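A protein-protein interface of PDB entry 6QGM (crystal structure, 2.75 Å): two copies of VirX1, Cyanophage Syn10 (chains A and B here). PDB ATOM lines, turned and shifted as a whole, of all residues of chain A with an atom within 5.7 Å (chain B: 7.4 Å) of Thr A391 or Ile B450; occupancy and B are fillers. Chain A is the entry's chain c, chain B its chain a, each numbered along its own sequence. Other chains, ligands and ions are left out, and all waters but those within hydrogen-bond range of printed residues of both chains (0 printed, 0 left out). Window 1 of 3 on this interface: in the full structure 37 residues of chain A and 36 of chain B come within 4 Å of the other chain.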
ATOM      1  N   ASN A 368      -0.877 -21.311 -15.646  1.00  0.00           N
ATOM      2  CA  ASN A 368      -0.770 -21.788 -17.056  1.00  0.00           C
ATOM      3  C   ASN A 368      -0.692 -23.326 -17.097  1.00  0.00           C
ATOM      4  O   ASN A 368      -1.246 -23.932 -18.052  1.00  0.00           O
ATOM      5  CB  ASN A 368       0.408 -21.131 -17.788  1.00  0.00           C
ATOM      6  CG  ASN A 368       0.191 -19.656 -18.030  1.00  0.00           C
ATOM      7  OD1 ASN A 368      -0.889 -19.137 -17.797  1.00  0.00           O
ATOM      8  ND2 ASN A 368       1.213 -18.971 -18.495  1.00  0.00           N
ATOM      9  N   TYR A 371      -4.176 -24.609 -16.093  1.00  0.00           N
ATOM     10  CA  TYR A 371      -5.038 -24.306 -17.263  1.00  0.00           C
ATOM     11  C   TYR A 371      -4.964 -25.480 -18.251  1.00  0.00           C
ATOM     12  O   TYR A 371      -6.023 -25.992 -18.655  1.00  0.00           O
ATOM     13  CB  TYR A 371      -4.651 -22.960 -17.889  1.00  0.00           C
ATOM     14  CG  TYR A 371      -5.398 -22.650 -19.158  1.00  0.00           C
ATOM     15  CD1 TYR A 371      -6.651 -22.056 -19.129  1.00  0.00           C
ATOM     16  CD2 TYR A 371      -4.868 -22.988 -20.394  1.00  0.00           C
ATOM     17  CE1 TYR A 371      -7.362 -21.801 -20.290  1.00  0.00           C
ATOM     18  CE2 TYR A 371      -5.558 -22.721 -21.567  1.00  0.00           C
ATOM     19  CZ  TYR A 371      -6.812 -22.136 -21.515  1.00  0.00           C
ATOM     20  OH  TYR A 371      -7.497 -21.891 -22.668  1.00  0.00           O
ATOM     21  N   LEU A 372      -3.753 -25.922 -18.593  1.00  0.00           N
ATOM     22  CA  LEU A 372      -3.537 -27.017 -19.576  1.00  0.00           C
ATOM     23  C   LEU A 372      -3.980 -28.367 -18.993  1.00  0.00           C
ATOM     24  O   LEU A 372      -4.556 -29.184 -19.748  1.00  0.00           O
ATOM     25  CB  LEU A 372      -2.059 -27.048 -19.978  1.00  0.00           C
ATOM     26  CG  LEU A 372      -1.592 -25.906 -20.871  1.00  0.00           C
ATOM     27  CD1 LEU A 372      -0.112 -26.084 -21.213  1.00  0.00           C
ATOM     28  CD2 LEU A 372      -2.450 -25.818 -22.126  1.00  0.00           C
ATOM     29  N   GLU A 384       0.542 -27.270 -27.184  1.00  0.00           N
ATOM     30  CA  GLU A 384       0.152 -26.583 -25.916  1.00  0.00           C
ATOM     31  C   GLU A 384       1.413 -26.258 -25.096  1.00  0.00           C
ATOM     32  O   GLU A 384       1.519 -25.127 -24.580  1.00  0.00           O
ATOM     33  CB  GLU A 384      -0.881 -27.413 -25.146  1.00  0.00           C
ATOM     34  CG  GLU A 384      -2.235 -27.489 -25.849  1.00  0.00           C
ATOM     35  CD  GLU A 384      -3.192 -28.593 -25.397  1.00  0.00           C
ATOM     36  OE1 GLU A 384      -3.975 -28.348 -24.428  1.00  0.00           O
ATOM     37  OE2 GLU A 384      -3.176 -29.691 -26.028  1.00  0.00           O
ATOM     38  N   ASP A 386       4.507 -25.906 -26.237  1.00  0.00           N
ATOM     39  CA  ASP A 386       5.170 -24.840 -27.038  1.00  0.00           C
ATOM     40  C   ASP A 386       4.471 -23.496 -26.750  1.00  0.00           C
ATOM     41  O   ASP A 386       5.172 -22.490 -26.572  1.00  0.00           O
ATOM     42  CB  ASP A 386       5.217 -25.230 -28.520  1.00  0.00           C
ATOM     43  CG  ASP A 386       6.181 -26.373 -28.812  1.00  0.00           C
ATOM     44  OD1 ASP A 386       6.946 -26.725 -27.908  1.00  0.00           O
ATOM     45  OD2 ASP A 386       6.165 -26.910 -29.947  1.00  0.00           O
ATOM     46  N   GLY A 387       3.143 -23.503 -26.665  1.00  0.00           N
ATOM     47  CA  GLY A 387       2.320 -22.338 -26.288  1.00  0.00           C
ATOM     48  C   GLY A 387       2.651 -21.836 -24.897  1.00  0.00           C
ATOM     49  O   GLY A 387       2.727 -20.596 -24.710  1.00  0.00           O
ATOM     50  N   PHE A 388       2.820 -22.761 -23.945  1.00  0.00           N
ATOM     51  CA  PHE A 388       3.205 -22.485 -22.533  1.00  0.00           C
ATOM     52  C   PHE A 388       4.554 -21.757 -22.504  1.00  0.00           C
ATOM     53  O   PHE A 388       4.698 -20.733 -21.792  1.00  0.00           O
ATOM     54  CB  PHE A 388       3.262 -23.797 -21.755  1.00  0.00           C
ATOM     55  CG  PHE A 388       3.654 -23.645 -20.311  1.00  0.00           C
ATOM     56  CD1 PHE A 388       4.991 -23.537 -19.941  1.00  0.00           C
ATOM     57  CD2 PHE A 388       2.680 -23.651 -19.326  1.00  0.00           C
ATOM     58  CE1 PHE A 388       5.338 -23.372 -18.613  1.00  0.00           C
ATOM     59  CE2 PHE A 388       3.027 -23.530 -17.991  1.00  0.00           C
ATOM     60  CZ  PHE A 388       4.354 -23.383 -17.640  1.00  0.00           C
ATOM     61  N   ASN A 389       5.525 -22.294 -23.254  1.00  0.00           N
ATOM     62  CA  ASN A 389       6.892 -21.731 -23.376  1.00  0.00           C
ATOM     63  C   ASN A 389       6.785 -20.327 -23.973  1.00  0.00           C
ATOM     64  O   ASN A 389       7.365 -19.404 -23.387  1.00  0.00           O
ATOM     65  CB  ASN A 389       7.808 -22.651 -24.180  1.00  0.00           C
ATOM     66  CG  ASN A 389       8.234 -23.887 -23.425  1.00  0.00           C
ATOM     67  OD1 ASN A 389       8.138 -23.936 -22.204  1.00  0.00           O
ATOM     68  ND2 ASN A 389       8.715 -24.882 -24.143  1.00  0.00           N
ATOM     69  N   TYR A 390       6.030 -20.160 -25.056  1.00  0.00           N
ATOM     70  CA  TYR A 390       5.869 -18.846 -25.717  1.00  0.00           C
ATOM     71  C   TYR A 390       5.266 -17.848 -24.723  1.00  0.00           C
ATOM     72  O   TYR A 390       5.849 -16.765 -24.537  1.00  0.00           O
ATOM     73  CB  TYR A 390       5.037 -18.925 -27.000  1.00  0.00           C
ATOM     74  CG  TYR A 390       4.904 -17.578 -27.665  1.00  0.00           C
ATOM     75  CD1 TYR A 390       5.943 -17.055 -28.421  1.00  0.00           C
ATOM     76  CD2 TYR A 390       3.773 -16.797 -27.500  1.00  0.00           C
ATOM     77  CE1 TYR A 390       5.845 -15.817 -29.037  1.00  0.00           C
ATOM     78  CE2 TYR A 390       3.658 -15.560 -28.108  1.00  0.00           C
ATOM     79  CZ  TYR A 390       4.699 -15.063 -28.878  1.00  0.00           C
ATOM     80  OH  TYR A 390       4.593 -13.834 -29.464  1.00  0.00           O
ATOM     81  N   THR A 391       4.137 -18.192 -24.108  1.00  0.00           N
ATOM     82  CA  THR A 391       3.406 -17.256 -23.218  1.00  0.00           C
ATOM     83  C   THR A 391       4.341 -16.773 -22.106  1.00  0.00           C
ATOM     84  O   THR A 391       4.373 -15.572 -21.851  1.00  0.00           O
ATOM     85  CB  THR A 391       2.145 -17.875 -22.619  1.00  0.00           C
ATOM     86  OG1 THR A 391       2.584 -19.046 -21.946  1.00  0.00           O
ATOM     87  CG2 THR A 391       1.087 -18.197 -23.647  1.00  0.00           C
ATOM     88  N   CYS A 392       5.086 -17.668 -21.475  1.00  0.00           N
ATOM     89  CA  CYS A 392       5.795 -17.333 -20.222  1.00  0.00           C
ATOM     90  C   CYS A 392       7.152 -16.697 -20.557  1.00  0.00           C
ATOM     91  O   CYS A 392       7.621 -15.864 -19.764  1.00  0.00           O
ATOM     92  CB  CYS A 392       5.865 -18.559 -19.326  1.00  0.00           C
ATOM     93  SG  CYS A 392       7.428 -19.453 -19.425  1.00  0.00           S
ATOM     94  N   ASP A 393       7.726 -17.036 -21.712  1.00  0.00           N
ATOM     95  CA  ASP A 393       8.899 -16.338 -22.304  1.00  0.00           C
ATOM     96  C   ASP A 393       8.537 -14.883 -22.641  1.00  0.00           C
ATOM     97  O   ASP A 393       9.270 -13.972 -22.208  1.00  0.00           O
ATOM     98  CB  ASP A 393       9.382 -17.047 -23.571  1.00  0.00           C
ATOM     99  CG  ASP A 393      10.688 -16.495 -24.097  1.00  0.00           C
ATOM    100  OD1 ASP A 393      11.733 -16.780 -23.464  1.00  0.00           O
ATOM    101  OD2 ASP A 393      10.646 -15.743 -25.104  1.00  0.00           O
ATOM    102  N   HIS A 394       7.450 -14.672 -23.388  1.00  0.00           N
ATOM    103  CA  HIS A 394       6.956 -13.321 -23.760  1.00  0.00           C
ATOM    104  C   HIS A 394       6.855 -12.446 -22.504  1.00  0.00           C
ATOM    105  O   HIS A 394       7.284 -11.277 -22.541  1.00  0.00           O
ATOM    106  CB  HIS A 394       5.607 -13.378 -24.496  1.00  0.00           C
ATOM    107  CG  HIS A 394       5.349 -12.153 -25.296  1.00  0.00           C
ATOM    108  ND1 HIS A 394       4.956 -10.954 -24.708  1.00  0.00           N
ATOM    109  CD2 HIS A 394       5.474 -11.908 -26.619  1.00  0.00           C
ATOM    110  CE1 HIS A 394       4.838 -10.027 -25.640  1.00  0.00           C
ATOM    111  NE2 HIS A 394       5.150 -10.583 -26.823  1.00  0.00           N
ATOM    112  N   GLN A 395       6.301 -13.004 -21.430  1.00  0.00           N
ATOM    113  CA  GLN A 395       5.959 -12.271 -20.186  1.00  0.00           C
ATOM    114  C   GLN A 395       7.241 -11.788 -19.512  1.00  0.00           C
ATOM    115  O   GLN A 395       7.313 -10.597 -19.179  1.00  0.00           O
ATOM    116  CB  GLN A 395       5.147 -13.163 -19.254  1.00  0.00           C
ATOM    117  CG  GLN A 395       5.058 -12.631 -17.838  1.00  0.00           C
ATOM    118  CD  GLN A 395       3.707 -12.836 -17.214  1.00  0.00           C
ATOM    119  OE1 GLN A 395       3.587 -13.550 -16.226  1.00  0.00           O
ATOM    120  NE2 GLN A 395       2.699 -12.190 -17.778  1.00  0.00           N
ATOM    121  N   ILE A 396       8.216 -12.676 -19.317  1.00  0.00           N
ATOM    122  CA  ILE A 396       9.459 -12.335 -18.576  1.00  0.00           C
ATOM    123  C   ILE A 396      10.297 -11.363 -19.419  1.00  0.00           C
ATOM    124  O   ILE A 396      10.984 -10.518 -18.822  1.00  0.00           O
ATOM    125  CB  ILE A 396      10.228 -13.596 -18.142  1.00  0.00           C
ATOM    126  CG1 ILE A 396      11.199 -13.274 -16.999  1.00  0.00           C
ATOM    127  CG2 ILE A 396      10.923 -14.252 -19.313  1.00  0.00           C
ATOM    128  CD1 ILE A 396      11.769 -14.481 -16.333  1.00  0.00           C
ATOM    129  N   TYR B 409      -3.708 -30.714 -32.249  1.00  0.00           N
ATOM    130  CA  TYR B 409      -4.547 -30.590 -31.029  1.00  0.00           C
ATOM    131  C   TYR B 409      -5.355 -31.869 -30.796  1.00  0.00           C
ATOM    132  O   TYR B 409      -6.081 -31.898 -29.795  1.00  0.00           O
ATOM    133  CB  TYR B 409      -5.436 -29.349 -31.137  1.00  0.00           C
ATOM    134  CG  TYR B 409      -4.653 -28.074 -31.003  1.00  0.00           C
ATOM    135  CD1 TYR B 409      -4.150 -27.689 -29.768  1.00  0.00           C
ATOM    136  CD2 TYR B 409      -4.371 -27.279 -32.104  1.00  0.00           C
ATOM    137  CE1 TYR B 409      -3.394 -26.538 -29.625  1.00  0.00           C
ATOM    138  CE2 TYR B 409      -3.646 -26.106 -31.963  1.00  0.00           C
ATOM    139  CZ  TYR B 409      -3.148 -25.743 -30.727  1.00  0.00           C
ATOM    140  OH  TYR B 409      -2.429 -24.605 -30.575  1.00  0.00           O
ATOM    141  N   MET B 428       5.575 -24.487 -33.995  1.00  0.00           N
ATOM    142  CA  MET B 428       5.848 -23.065 -33.671  1.00  0.00           C
ATOM    143  C   MET B 428       7.350 -22.820 -33.625  1.00  0.00           C
ATOM    144  O   MET B 428       7.811 -22.080 -32.761  1.00  0.00           O
ATOM    145  CB  MET B 428       5.268 -22.710 -32.297  1.00  0.00           C
ATOM    146  CG  MET B 428       3.776 -22.629 -32.248  1.00  0.00           C
ATOM    147  SD  MET B 428       3.111 -22.520 -30.564  1.00  0.00           S
ATOM    148  CE  MET B 428       4.029 -21.135 -29.909  1.00  0.00           C
ATOM    149  N   MET B 432      10.025 -18.613 -30.746  1.00  0.00           N
ATOM    150  CA  MET B 432      10.898 -18.270 -29.591  1.00  0.00           C
ATOM    151  C   MET B 432      11.969 -17.270 -30.040  1.00  0.00           C
ATOM    152  O   MET B 432      12.733 -16.787 -29.170  1.00  0.00           O
ATOM    153  CB  MET B 432      11.579 -19.504 -29.002  1.00  0.00           C
ATOM    154  CG  MET B 432      10.616 -20.473 -28.289  1.00  0.00           C
ATOM    155  SD  MET B 432       9.427 -19.723 -27.113  1.00  0.00           S
ATOM    156  CE  MET B 432      10.221 -20.093 -25.548  1.00  0.00           C
ATOM    157  N   GLN B 443       1.150 -18.793 -32.514  1.00  0.00           N
ATOM    158  CA  GLN B 443       1.613 -17.863 -31.449  1.00  0.00           C
ATOM    159  C   GLN B 443       0.398 -17.159 -30.836  1.00  0.00           C
ATOM    160  O   GLN B 443       0.335 -17.065 -29.588  1.00  0.00           O
ATOM    161  CB  GLN B 443       2.598 -16.842 -32.034  1.00  0.00           C
ATOM    162  CG  GLN B 443       3.920 -17.447 -32.454  1.00  0.00           C
ATOM    163  CD  GLN B 443       4.621 -16.900 -33.678  1.00  0.00           C
ATOM    164  OE1 GLN B 443       5.211 -17.664 -34.437  1.00  0.00           O
ATOM    165  NE2 GLN B 443       4.607 -15.591 -33.870  1.00  0.00           N
ATOM    166  N   ASP B 444      -0.531 -16.703 -31.684  1.00  0.00           N
ATOM    167  CA  ASP B 444      -1.650 -15.811 -31.280  1.00  0.00           C
ATOM    168  C   ASP B 444      -2.695 -16.633 -30.534  1.00  0.00           C
ATOM    169  O   ASP B 444      -3.222 -16.136 -29.535  1.00  0.00           O
ATOM    170  CB  ASP B 444      -2.251 -15.075 -32.485  1.00  0.00           C
ATOM    171  CG  ASP B 444      -1.316 -14.093 -33.144  1.00  0.00           C
ATOM    172  OD1 ASP B 444      -0.284 -13.762 -32.500  1.00  0.00           O
ATOM    173  OD2 ASP B 444      -1.622 -13.687 -34.300  1.00  0.00           O
ATOM    174  N   LEU B 445      -2.973 -17.846 -31.006  1.00  0.00           N
ATOM    175  CA  LEU B 445      -3.933 -18.782 -30.367  1.00  0.00           C
ATOM    176  C   LEU B 445      -3.398 -19.162 -28.989  1.00  0.00           C
ATOM    177  O   LEU B 445      -4.201 -19.286 -28.071  1.00  0.00           O
ATOM    178  CB  LEU B 445      -4.106 -20.021 -31.251  1.00  0.00           C
ATOM    179  CG  LEU B 445      -5.100 -21.057 -30.735  1.00  0.00           C
ATOM    180  CD1 LEU B 445      -6.500 -20.476 -30.644  1.00  0.00           C
ATOM    181  CD2 LEU B 445      -5.098 -22.276 -31.641  1.00  0.00           C
ATOM    182  N   SER B 446      -2.081 -19.358 -28.874  1.00  0.00           N
ATOM    183  CA  SER B 446      -1.406 -19.775 -27.619  1.00  0.00           C
ATOM    184  C   SER B 446      -1.542 -18.647 -26.603  1.00  0.00           C
ATOM    185  O   SER B 446      -1.921 -18.928 -25.455  1.00  0.00           O
ATOM    186  CB  SER B 446       0.040 -20.148 -27.860  1.00  0.00           C
ATOM    187  OG  SER B 446       0.144 -21.413 -28.521  1.00  0.00           O
ATOM    188  N   THR B 447      -1.272 -17.417 -27.045  1.00  0.00           N
ATOM    189  CA  THR B 447      -1.437 -16.156 -26.265  1.00  0.00           C
ATOM    190  C   THR B 447      -2.896 -15.978 -25.825  1.00  0.00           C
ATOM    191  O   THR B 447      -3.116 -15.613 -24.655  1.00  0.00           O
ATOM    192  CB  THR B 447      -1.005 -14.948 -27.095  1.00  0.00           C
ATOM    193  OG1 THR B 447       0.415 -15.052 -27.155  1.00  0.00           O
ATOM    194  CG2 THR B 447      -1.466 -13.622 -26.525  1.00  0.00           C
ATOM    195  N   ASP B 448      -3.850 -16.204 -26.734  1.00  0.00           N
ATOM    196  CA  ASP B 448      -5.288 -15.952 -26.471  1.00  0.00           C
ATOM    197  C   ASP B 448      -5.787 -16.954 -25.429  1.00  0.00           C
ATOM    198  O   ASP B 448      -6.510 -16.519 -24.514  1.00  0.00           O
ATOM    199  CB  ASP B 448      -6.105 -15.963 -27.767  1.00  0.00           C
ATOM    200  CG  ASP B 448      -5.869 -14.741 -28.631  1.00  0.00           C
ATOM    201  OD1 ASP B 448      -5.098 -13.853 -28.194  1.00  0.00           O
ATOM    202  OD2 ASP B 448      -6.430 -14.693 -29.749  1.00  0.00           O
ATOM    203  N   THR B 449      -5.400 -18.229 -25.549  1.00  0.00           N
ATOM    204  CA  THR B 449      -5.939 -19.359 -24.748  1.00  0.00           C
ATOM    205  C   THR B 449      -5.206 -19.406 -23.402  1.00  0.00           C
ATOM    206  O   THR B 449      -5.851 -19.110 -22.381  1.00  0.00           O
ATOM    207  CB  THR B 449      -5.877 -20.677 -25.527  1.00  0.00           C
ATOM    208  OG1 THR B 449      -4.516 -20.876 -25.907  1.00  0.00           O
ATOM    209  CG2 THR B 449      -6.783 -20.684 -26.742  1.00  0.00           C
ATOM    210  N   ILE B 450      -3.914 -19.729 -23.391  1.00  0.00           N
ATOM    211  CA  ILE B 450      -3.124 -19.878 -22.133  1.00  0.00           C
ATOM    212  C   ILE B 450      -2.914 -18.496 -21.497  1.00  0.00           C
ATOM    213  O   ILE B 450      -3.055 -18.394 -20.263  1.00  0.00           O
ATOM    214  CB  ILE B 450      -1.787 -20.592 -22.410  1.00  0.00           C
ATOM    215  CG1 ILE B 450      -1.979 -21.919 -23.151  1.00  0.00           C
ATOM    216  CG2 ILE B 450      -0.996 -20.777 -21.121  1.00  0.00           C
ATOM    217  CD1 ILE B 450      -0.713 -22.396 -23.850  1.00  0.00           C
ATOM    218  N   GLY B 451      -2.596 -17.469 -22.292  1.00  0.00           N
ATOM    219  CA  GLY B 451      -2.268 -16.117 -21.789  1.00  0.00           C
ATOM    220  C   GLY B 451      -3.481 -15.372 -21.248  1.00  0.00           C
ATOM    221  O   GLY B 451      -3.452 -15.002 -20.048  1.00  0.00           O
ATOM    222  N   LEU B 452      -4.505 -15.195 -22.095  1.00  0.00           N
ATOM    223  CA  LEU B 452      -5.693 -14.321 -21.877  1.00  0.00           C
ATOM    224  C   LEU B 452      -6.987 -15.123 -21.591  1.00  0.00           C
ATOM    225  O   LEU B 452      -8.031 -14.481 -21.345  1.00  0.00           O
ATOM    226  CB  LEU B 452      -5.885 -13.457 -23.130  1.00  0.00           C
ATOM    227  CG  LEU B 452      -4.775 -12.444 -23.411  1.00  0.00           C
ATOM    228  CD1 LEU B 452      -4.992 -11.736 -24.740  1.00  0.00           C
ATOM    229  CD2 LEU B 452      -4.641 -11.445 -22.277  1.00  0.00           C
ATOM    230  N   ASN B 453      -6.945 -16.464 -21.672  1.00  0.00           N
ATOM    231  CA  ASN B 453      -8.063 -17.390 -21.355  1.00  0.00           C
ATOM    232  C   ASN B 453      -9.310 -17.016 -22.166  1.00  0.00           C
ATOM    233  O   ASN B 453     -10.417 -17.007 -21.599  1.00  0.00           O
ATOM    234  CB  ASN B 453      -8.318 -17.418 -19.845  1.00  0.00           C
ATOM    235  CG  ASN B 453      -7.162 -17.955 -19.032  1.00  0.00           C
ATOM    236  OD1 ASN B 453      -7.097 -17.707 -17.828  1.00  0.00           O
ATOM    237  ND2 ASN B 453      -6.237 -18.660 -19.678  1.00  0.00           N
ATOM    238  N   THR B 454      -9.156 -16.780 -23.463  1.00  0.00           N
ATOM    239  CA  THR B 454     -10.223 -16.246 -24.345  1.00  0.00           C
ATOM    240  C   THR B 454     -10.110 -16.829 -25.753  1.00  0.00           C
ATOM    241  O   THR B 454      -8.996 -17.144 -26.172  1.00  0.00           O
ATOM    242  CB  THR B 454     -10.153 -14.714 -24.421  1.00  0.00           C
ATOM    243  OG1 THR B 454     -11.370 -14.236 -24.992  1.00  0.00           O
ATOM    244  CG2 THR B 454      -8.993 -14.201 -25.245  1.00  0.00           C
ATOM    245  N   PRO B 473     -12.049 -21.977 -23.919  1.00  0.00           N
ATOM    246  CA  PRO B 473     -11.265 -20.770 -23.662  1.00  0.00           C
ATOM    247  C   PRO B 473     -10.836 -20.657 -22.192  1.00  0.00           C
ATOM    248  O   PRO B 473      -9.685 -20.305 -21.948  1.00  0.00           O
ATOM    249  CB  PRO B 473     -12.179 -19.605 -24.075  1.00  0.00           C
ATOM    250  CG  PRO B 473     -13.585 -20.190 -24.177  1.00  0.00           C
ATOM    251  CD  PRO B 473     -13.406 -21.670 -24.407  1.00  0.00           C
ATOM    252  N   LEU B 479     -12.092 -20.467 -12.572  1.00  0.00           N
ATOM    253  CA  LEU B 479     -11.289 -19.414 -13.247  1.00  0.00           C
ATOM    254  C   LEU B 479     -12.187 -18.238 -13.643  1.00  0.00           C
ATOM    255  O   LEU B 479     -11.814 -17.074 -13.341  1.00  0.00           O
ATOM    256  CB  LEU B 479     -10.620 -20.078 -14.451  1.00  0.00           C
ATOM    257  CG  LEU B 479      -9.707 -19.183 -15.265  1.00  0.00           C
ATOM    258  CD1 LEU B 479      -8.753 -18.418 -14.351  1.00  0.00           C
ATOM    259  CD2 LEU B 479      -8.955 -20.028 -16.288  1.00  0.00           C
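The backbone carbonyl oxygen of Thr B449 sits at hydrogen-bond distance from the side-chain hydroxyl of Tyr A371 (3.2 Å). The side-chain amide oxygen (OD1) of Asn A368 sits close to the backbone carbonyl oxygen (O) of Ile B450 (3.4 Å). The backbone carbonyl oxygen (O) of Pro B473 lies within hydrogen-bond range of the side-chain hydroxyl (OH) of Tyr A371 (2.8 Å).
The backbone carbonyl oxygen of Gln B443 lies within hydrogen-bond range of the side-chain hydroxyl of Thr B447 (3.2 Å). The backbone carbonyl oxygen of Leu B445 sits at hydrogen-bond distance from the side-chain hydroxyl of Thr B449 (2.7 Å). OG1 of Thr B449 lies within hydrogen-bond range of O of Ser B446, at 3.3 Å. O of Thr B447 lies within hydrogen-bond range of N of Leu B452, at 2.9 Å. The backbone carbonyl oxygen (O) of Asp B448 lies within hydrogen-bond range of the backbone NH (N) of Asn B453, at 2.9 Å. ND2 of Asn B453 is in hydrogen-bond range of O of Thr B449 (2.8 Å).
Among the printed residues, merely in contact across the chains: Tyr A371 with Ile B450, Tyr A371 with Asn B453, Glu A384 with Ile B450, Asp A386 with Met B428, Gly A387 with Ser B446, Gly A387 with Ile B450, Phe A388 with Ile B450, Asn A389 with Met B432, Tyr A390 with Met B428, Tyr A390 with Met B432, Tyr A390 with Gln B443, Tyr A390 with Thr B447, Thr A391 with Ser B446, Thr A391 with Ile B450, Thr A391 with Gly B451 and Asp A393 with Met B432.
Printed residues of chain B within 4 Å of Thr A391: Ser B446, Ile B450 and Gly B451. Of the printed residues of chain A, Met B428 touches Asp A386 (3.8 Å) and Tyr A390 (3.8 Å). Asp B444 touches none of the printed residues of chain A. Ile B450 touches just these residues of chain A: Asn A368, Tyr A371, Glu A384, Gly A387, Phe A388 and Thr A391. Of the printed residues of chain A, Asn B453 touches Tyr A371 (3.4 Å). Thr B454 touches none of the printed residues of chain A. The nearest printed residue of chain B that does not touch Thr A391 is Thr B447 (4.2 Å). The nearest residue of chain A that does not touch Ile B450 is Leu A372 (4.1 Å). The nearest printed residue of chain A that does not touch Pro B473 is Leu A372 (8.8 Å).
Hydrophobic or aromatic side chains of chain A that line the printed part of chain B: Tyr A371 and Tyr A390. Of the 17 printed residues of chain B, 10 touch a printed residue of chain A. Among the printed residues, 19 pairs touch across the chains.
No position is printed for both chains.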
